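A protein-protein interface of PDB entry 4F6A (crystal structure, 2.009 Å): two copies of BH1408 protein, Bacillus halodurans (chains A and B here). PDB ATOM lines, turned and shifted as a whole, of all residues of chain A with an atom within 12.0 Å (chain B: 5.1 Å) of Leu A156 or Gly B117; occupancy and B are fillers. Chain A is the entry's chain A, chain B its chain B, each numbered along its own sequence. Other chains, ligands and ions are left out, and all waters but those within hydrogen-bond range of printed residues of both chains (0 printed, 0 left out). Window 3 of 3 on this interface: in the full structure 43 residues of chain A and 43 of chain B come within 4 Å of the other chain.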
ATOM      1  N   ARG A  29      11.456 -27.652  -8.552  1.00  0.00           N
ATOM      2  CA  ARG A  29      10.190 -26.928  -8.615  1.00  0.00           C
ATOM      3  C   ARG A  29       9.900 -26.217  -7.285  1.00  0.00           C
ATOM      4  O   ARG A  29       8.926 -26.520  -6.605  1.00  0.00           O
ATOM      5  CB  ARG A  29       9.030 -27.864  -8.986  1.00  0.00           C
ATOM      6  CG  ARG A  29       9.084 -28.435 -10.423  1.00  0.00           C
ATOM      7  CD  ARG A  29       9.018 -27.349 -11.497  1.00  0.00           C
ATOM      8  NE  ARG A  29       7.824 -26.497 -11.424  1.00  0.00           N
ATOM      9  CZ  ARG A  29       6.746 -26.641 -12.197  1.00  0.00           C
ATOM     10  NH1 ARG A  29       6.690 -27.615 -13.103  1.00  0.00           N
ATOM     11  NH2 ARG A  29       5.727 -25.800 -12.079  1.00  0.00           N
ATOM     12  N   ASP A  31       8.679 -23.496  -6.866  1.00  0.00           N
ATOM     13  CA  ASP A  31       7.414 -22.762  -6.945  1.00  0.00           C
ATOM     14  C   ASP A  31       6.280 -23.597  -6.356  1.00  0.00           C
ATOM     15  O   ASP A  31       5.230 -23.076  -5.977  1.00  0.00           O
ATOM     16  CB  ASP A  31       7.096 -22.364  -8.398  1.00  0.00           C
ATOM     17  CG  ASP A  31       7.089 -23.556  -9.354  1.00  0.00           C
ATOM     18  OD1 ASP A  31       7.885 -24.499  -9.157  1.00  0.00           O
ATOM     19  OD2 ASP A  31       6.278 -23.559 -10.306  1.00  0.00           O
ATOM     20  N   ILE A  32       6.499 -24.905  -6.274  1.00  0.00           N
ATOM     21  CA  ILE A  32       5.484 -25.815  -5.751  1.00  0.00           C
ATOM     22  C   ILE A  32       5.885 -26.400  -4.395  1.00  0.00           C
ATOM     23  O   ILE A  32       5.084 -26.405  -3.459  1.00  0.00           O
ATOM     24  CB  ILE A  32       5.199 -26.954  -6.757  1.00  0.00           C
ATOM     25  CG1 ILE A  32       4.560 -26.391  -8.033  1.00  0.00           C
ATOM     26  CG2 ILE A  32       4.303 -28.032  -6.143  1.00  0.00           C
ATOM     27  CD1 ILE A  32       4.459 -27.418  -9.153  1.00  0.00           C
ATOM     28  N   MET A 152      -1.055 -30.533 -17.536  1.00  0.00           N
ATOM     29  CA  MET A 152      -0.349 -29.493 -18.261  1.00  0.00           C
ATOM     30  C   MET A 152      -0.542 -28.155 -17.571  1.00  0.00           C
ATOM     31  O   MET A 152      -1.519 -27.971 -16.847  1.00  0.00           O
ATOM     32  CB  MET A 152      -0.785 -29.476 -19.718  1.00  0.00           C
ATOM     33  CG  MET A 152      -0.067 -30.634 -20.480  1.00  0.00           C
ATOM     34  SD  MET A 152      -0.588 -30.662 -22.290  1.00  0.00           S
ATOM     35  CE  MET A 152       0.808 -29.436 -22.959  1.00  0.00           C
ATOM     36  N   GLU A 153       0.402 -27.240 -17.771  1.00  0.00           N
ATOM     37  CA  GLU A 153       0.402 -25.999 -17.010  1.00  0.00           C
ATOM     38  C   GLU A 153       0.832 -24.816 -17.862  1.00  0.00           C
ATOM     39  O   GLU A 153       1.617 -24.954 -18.802  1.00  0.00           O
ATOM     40  CB  GLU A 153       1.327 -26.113 -15.780  1.00  0.00           C
ATOM     41  CG  GLU A 153       2.820 -26.242 -16.156  1.00  0.00           C
ATOM     42  CD  GLU A 153       3.748 -26.425 -14.945  1.00  0.00           C
ATOM     43  OE1 GLU A 153       3.398 -25.983 -13.834  1.00  0.00           O
ATOM     44  OE2 GLU A 153       4.830 -27.025 -15.108  1.00  0.00           O
ATOM     45  N   LEU A 154       0.288 -23.653 -17.533  1.00  0.00           N
ATOM     46  CA  LEU A 154       0.698 -22.407 -18.151  1.00  0.00           C
ATOM     47  C   LEU A 154       0.811 -21.365 -17.056  1.00  0.00           C
ATOM     48  O   LEU A 154      -0.204 -20.880 -16.572  1.00  0.00           O
ATOM     49  CB  LEU A 154      -0.349 -21.948 -19.159  1.00  0.00           C
ATOM     50  CG  LEU A 154      -0.027 -20.622 -19.853  1.00  0.00           C
ATOM     51  CD1 LEU A 154       1.223 -20.755 -20.718  1.00  0.00           C
ATOM     52  CD2 LEU A 154      -1.221 -20.141 -20.681  1.00  0.00           C
ATOM     53  N   PRO A 155       2.044 -21.017 -16.656  1.00  0.00           N
ATOM     54  CA  PRO A 155       2.250 -19.994 -15.622  1.00  0.00           C
ATOM     55  C   PRO A 155       1.776 -18.628 -16.104  1.00  0.00           C
ATOM     56  O   PRO A 155       1.961 -18.312 -17.279  1.00  0.00           O
ATOM     57  CB  PRO A 155       3.776 -19.979 -15.439  1.00  0.00           C
ATOM     58  CG  PRO A 155       4.244 -21.294 -15.982  1.00  0.00           C
ATOM     59  CD  PRO A 155       3.310 -21.609 -17.113  1.00  0.00           C
ATOM     60  N   LEU A 156       1.182 -17.828 -15.218  1.00  0.00           N
ATOM     61  CA  LEU A 156       0.671 -16.511 -15.606  1.00  0.00           C
ATOM     62  C   LEU A 156       1.475 -15.350 -15.016  1.00  0.00           C
ATOM     63  O   LEU A 156       2.358 -15.544 -14.181  1.00  0.00           O
ATOM     64  CB  LEU A 156      -0.808 -16.367 -15.234  1.00  0.00           C
ATOM     65  CG  LEU A 156      -1.805 -17.215 -16.028  1.00  0.00           C
ATOM     66  CD1 LEU A 156      -3.232 -16.768 -15.745  1.00  0.00           C
ATOM     67  CD2 LEU A 156      -1.518 -17.158 -17.530  1.00  0.00           C
ATOM     68  N   VAL B  89      -6.124 -21.664 -11.796  1.00  0.00           N
ATOM     69  CA  VAL B  89      -7.368 -21.975 -12.467  1.00  0.00           C
ATOM     70  C   VAL B  89      -7.194 -23.374 -13.032  1.00  0.00           C
ATOM     71  O   VAL B  89      -6.261 -23.619 -13.788  1.00  0.00           O
ATOM     72  CB  VAL B  89      -7.612 -21.010 -13.629  1.00  0.00           C
ATOM     73  CG1 VAL B  89      -8.765 -21.504 -14.486  1.00  0.00           C
ATOM     74  CG2 VAL B  89      -7.870 -19.594 -13.088  1.00  0.00           C
ATOM     75  N   ILE B 113     -10.293 -17.674 -20.599  1.00  0.00           N
ATOM     76  CA  ILE B 113      -9.824 -18.325 -19.380  1.00  0.00           C
ATOM     77  C   ILE B 113      -8.569 -17.630 -18.843  1.00  0.00           C
ATOM     78  O   ILE B 113      -8.436 -17.404 -17.636  1.00  0.00           O
ATOM     79  CB  ILE B 113      -9.555 -19.817 -19.624  1.00  0.00           C
ATOM     80  CG1 ILE B 113     -10.856 -20.508 -20.060  1.00  0.00           C
ATOM     81  CG2 ILE B 113      -9.005 -20.481 -18.366  1.00  0.00           C
ATOM     82  CD1 ILE B 113     -10.698 -21.990 -20.370  1.00  0.00           C
ATOM     83  N   ILE B 114      -7.657 -17.277 -19.743  1.00  0.00           N
ATOM     84  CA  ILE B 114      -6.471 -16.518 -19.349  1.00  0.00           C
ATOM     85  C   ILE B 114      -6.863 -15.188 -18.681  1.00  0.00           C
ATOM     86  O   ILE B 114      -6.310 -14.825 -17.637  1.00  0.00           O
ATOM     87  CB  ILE B 114      -5.535 -16.258 -20.547  1.00  0.00           C
ATOM     88  CG1 ILE B 114      -4.851 -17.560 -20.991  1.00  0.00           C
ATOM     89  CG2 ILE B 114      -4.483 -15.202 -20.194  1.00  0.00           C
ATOM     90  CD1 ILE B 114      -4.056 -17.415 -22.303  1.00  0.00           C
ATOM     91  N   SER B 115      -7.823 -14.479 -19.275  1.00  0.00           N
ATOM     92  CA  SER B 115      -8.297 -13.208 -18.722  1.00  0.00           C
ATOM     93  C   SER B 115      -8.845 -13.371 -17.318  1.00  0.00           C
ATOM     94  O   SER B 115      -8.597 -12.546 -16.439  1.00  0.00           O
ATOM     95  CB  SER B 115      -9.385 -12.599 -19.606  1.00  0.00           C
ATOM     96  OG  SER B 115      -8.858 -12.279 -20.878  1.00  0.00           O
ATOM     97  N   TYR B 116      -9.613 -14.433 -17.121  1.00  0.00           N
ATOM     98  CA  TYR B 116     -10.159 -14.733 -15.810  1.00  0.00           C
ATOM     99  C   TYR B 116      -9.024 -14.979 -14.806  1.00  0.00           C
ATOM    100  O   TYR B 116      -9.021 -14.414 -13.706  1.00  0.00           O
ATOM    101  CB  TYR B 116     -11.085 -15.942 -15.913  1.00  0.00           C
ATOM    102  CG  TYR B 116     -11.662 -16.416 -14.599  1.00  0.00           C
ATOM    103  CD1 TYR B 116     -11.016 -17.393 -13.846  1.00  0.00           C
ATOM    104  CD2 TYR B 116     -12.870 -15.916 -14.125  1.00  0.00           C
ATOM    105  CE1 TYR B 116     -11.545 -17.843 -12.644  1.00  0.00           C
ATOM    106  CE2 TYR B 116     -13.406 -16.360 -12.924  1.00  0.00           C
ATOM    107  CZ  TYR B 116     -12.739 -17.328 -12.191  1.00  0.00           C
ATOM    108  OH  TYR B 116     -13.260 -17.775 -10.998  1.00  0.00           O
ATOM    109  N   GLY B 117      -8.062 -15.809 -15.194  1.00  0.00           N
ATOM    110  CA  GLY B 117      -6.920 -16.112 -14.339  1.00  0.00           C
ATOM    111  C   GLY B 117      -6.170 -14.858 -13.917  1.00  0.00           C
ATOM    112  O   GLY B 117      -5.770 -14.704 -12.758  1.00  0.00           O
ATOM    113  N   LYS B 118      -5.994 -13.943 -14.862  1.00  0.00           N
ATOM    114  CA  LYS B 118      -5.285 -12.702 -14.586  1.00  0.00           C
ATOM    115  C   LYS B 118      -6.083 -11.818 -13.628  1.00  0.00           C
ATOM    116  O   LYS B 118      -5.515 -11.208 -12.718  1.00  0.00           O
ATOM    117  CB  LYS B 118      -4.975 -11.949 -15.880  1.00  0.00           C
ATOM    118  CG  LYS B 118      -3.891 -12.593 -16.744  1.00  0.00           C
ATOM    119  CD  LYS B 118      -3.564 -11.707 -17.945  1.00  0.00           C
ATOM    120  CE  LYS B 118      -2.499 -12.320 -18.850  1.00  0.00           C
ATOM    121  NZ  LYS B 118      -2.384 -11.573 -20.145  1.00  0.00           N
ATOM    122  N   ALA B 119      -7.398 -11.757 -13.832  1.00  0.00           N
ATOM    123  CA  ALA B 119      -8.254 -10.953 -12.963  1.00  0.00           C
ATOM    124  C   ALA B 119      -8.174 -11.476 -11.531  1.00  0.00           C
ATOM    125  O   ALA B 119      -8.194 -10.704 -10.578  1.00  0.00           O
ATOM    126  CB  ALA B 119      -9.698 -10.951 -13.459  1.00  0.00           C
ATOM    127  N   HIS B 120      -8.057 -12.793 -11.391  1.00  0.00           N
ATOM    128  CA  HIS B 120      -7.934 -13.403 -10.074  1.00  0.00           C
ATOM    129  C   HIS B 120      -6.486 -13.556  -9.620  1.00  0.00           C
ATOM    130  O   HIS B 120      -6.221 -14.166  -8.582  1.00  0.00           O
ATOM    131  CB  HIS B 120      -8.683 -14.735 -10.035  1.00  0.00           C
ATOM    132  CG  HIS B 120     -10.169 -14.568 -10.081  1.00  0.00           C
ATOM    133  ND1 HIS B 120     -10.924 -14.347  -8.948  1.00  0.00           N
ATOM    134  CD2 HIS B 120     -11.033 -14.537 -11.122  1.00  0.00           C
ATOM    135  CE1 HIS B 120     -12.194 -14.209  -9.288  1.00  0.00           C
ATOM    136  NE2 HIS B 120     -12.287 -14.316 -10.602  1.00  0.00           N
ATOM    137  N   GLN B 121      -5.566 -12.979 -10.394  1.00  0.00           N
ATOM    138  CA  GLN B 121      -4.133 -13.029 -10.098  1.00  0.00           C
ATOM    139  C   GLN B 121      -3.640 -14.424  -9.716  1.00  0.00           C
ATOM    140  O   GLN B 121      -2.993 -14.599  -8.682  1.00  0.00           O
ATOM    141  CB  GLN B 121      -3.783 -12.034  -8.986  1.00  0.00           C
ATOM    142  CG  GLN B 121      -4.284 -10.622  -9.244  1.00  0.00           C
ATOM    143  CD  GLN B 121      -4.001  -9.677  -8.081  1.00  0.00           C
ATOM    144  OE1 GLN B 121      -4.923  -9.124  -7.478  1.00  0.00           O
ATOM    145  NE2 GLN B 121      -2.722  -9.486  -7.766  1.00  0.00           N
ATOM    146  N   VAL B 122      -3.946 -15.422 -10.540  1.00  0.00           N
ATOM    147  CA  VAL B 122      -3.525 -16.776 -10.217  1.00  0.00           C
ATOM    148  C   VAL B 122      -2.090 -17.041 -10.672  1.00  0.00           C
ATOM    149  O   VAL B 122      -1.522 -16.273 -11.445  1.00  0.00           O
ATOM    150  CB  VAL B 122      -4.464 -17.833 -10.831  1.00  0.00           C
ATOM    151  CG1 VAL B 122      -5.907 -17.521 -10.467  1.00  0.00           C
ATOM    152  CG2 VAL B 122      -4.290 -17.888 -12.354  1.00  0.00           C
ATOM    153  N   ASP B 123      -1.513 -18.137 -10.191  1.00  0.00           N
ATOM    154  CA  ASP B 123      -0.146 -18.499 -10.543  1.00  0.00           C
ATOM    155  C   ASP B 123      -0.078 -19.187 -11.904  1.00  0.00           C
ATOM    156  O   ASP B 123       0.889 -19.021 -12.643  1.00  0.00           O
ATOM    157  CB  ASP B 123       0.460 -19.417  -9.469  1.00  0.00           C
ATOM    158  CG  ASP B 123       0.521 -18.754  -8.093  1.00  0.00           C
ATOM    159  OD1 ASP B 123       1.066 -17.631  -7.989  1.00  0.00           O
ATOM    160  OD2 ASP B 123       0.008 -19.350  -7.121  1.00  0.00           O
ATOM    161  N   ALA B 124      -1.108 -19.958 -12.240  1.00  0.00           N
ATOM    162  CA  ALA B 124      -1.046 -20.764 -13.448  1.00  0.00           C
ATOM    163  C   ALA B 124      -2.417 -21.266 -13.849  1.00  0.00           C
ATOM    164  O   ALA B 124      -3.334 -21.323 -13.040  1.00  0.00           O
ATOM    165  CB  ALA B 124      -0.117 -21.961 -13.223  1.00  0.00           C
ATOM    166  N   ILE B 125      -2.535 -21.637 -15.113  1.00  0.00           N
ATOM    167  CA  ILE B 125      -3.668 -22.408 -15.574  1.00  0.00           C
ATOM    168  C   ILE B 125      -3.192 -23.856 -15.681  1.00  0.00           C
ATOM    169  O   ILE B 125      -2.082 -24.108 -16.161  1.00  0.00           O
ATOM    170  CB  ILE B 125      -4.117 -21.916 -16.952  1.00  0.00           C
ATOM    171  CG1 ILE B 125      -4.541 -20.449 -16.849  1.00  0.00           C
ATOM    172  CG2 ILE B 125      -5.263 -22.781 -17.477  1.00  0.00           C
ATOM    173  CD1 ILE B 125      -4.944 -19.837 -18.167  1.00  0.00           C
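Of chain B, only Gly B117 (3.95 Å), Val B122 (3.7 Å) and Asp B123 (2.9 Å) come within 4 Å of Leu A156.
Of the printed residues of chain A, Gly B117 touches Leu A156.
No residue of chain A comes within 4 Å of Tyr B116.
Lys B118 touches none of the printed residues of chain A.
Gln B121 touches none of the printed residues of chain A.
Ala B124 touches just these residues of chain A: Leu A154 and Pro A155.
Ile B125 touches three residues of chain A.
Of the printed residues of chain B, Pro A155 touches Asp B123 and Ala B124.
Printed residues of chain B within 4 Å of Leu A154: Ala B124 and Ile B125.
Printed residues of chain A within 4 Å of Asp B123: Pro A155 (3.4 Å) and Leu A156 (2.9 Å).
Arg A29 touches none of the printed residues of chain B.
The nearest residue of chain A that does not touch Gly B117 is Leu A154 (8.5 Å).
The nearest printed residue of chain B that does not touch Glu A153 is Ala B124 (5.1 Å).
OE2 of Glu A153 lies within salt-bridge range of NH1 of Arg A29, 2.8 Å away.
O of Gly B117 is in hydrogen-bond range of N of Val B122 (3.0 Å).
O of Ala B124 lies within hydrogen-bond range of N of Val B89.
O of Ile B125 sits at hydrogen-bond distance from N of Leu A154 (2.8 Å).
The backbone NH (N) of Leu A156 sits at hydrogen-bond distance from the backbone carbonyl oxygen (O) of Asp B123 (2.9 Å).
Hydrophobic or aromatic side chains of chain B that line the printed part of chain A: Val B122 and Ala B124.
Of the 8 printed residues of chain A, 5 touch a printed residue of chain B.
Hydrophobic or aromatic side chains of chain A that line the printed part of chain B: Leu A156.
Along chain A the printed residues that touch a printed residue of chain B span positions 152 to 156.
Among the printed residues, no Asp or Glu carboxylate lies within 4 Å of a Lys or Arg side-chain nitrogen of the other chain.
No position is printed for both chains.
Of the 9 pairs that touch across the chains among the printed residues, none has its exchanged pair printed and touching as well.
Among the printed residues, pairs that only touch across the chains: Glu A153 with Ile B125 (3.2 Å), Leu A154 with Ala B124 (3.2 Å), Pro A155 with Asp B123 (3.4 Å), Leu A156 with Val B122 (3.7 Å), Pro A155 with Ala B124 (3.9 Å), Leu A156 with Gly B117 (3.95 Å) and Met A152 with Ile B125 (3.96 Å).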
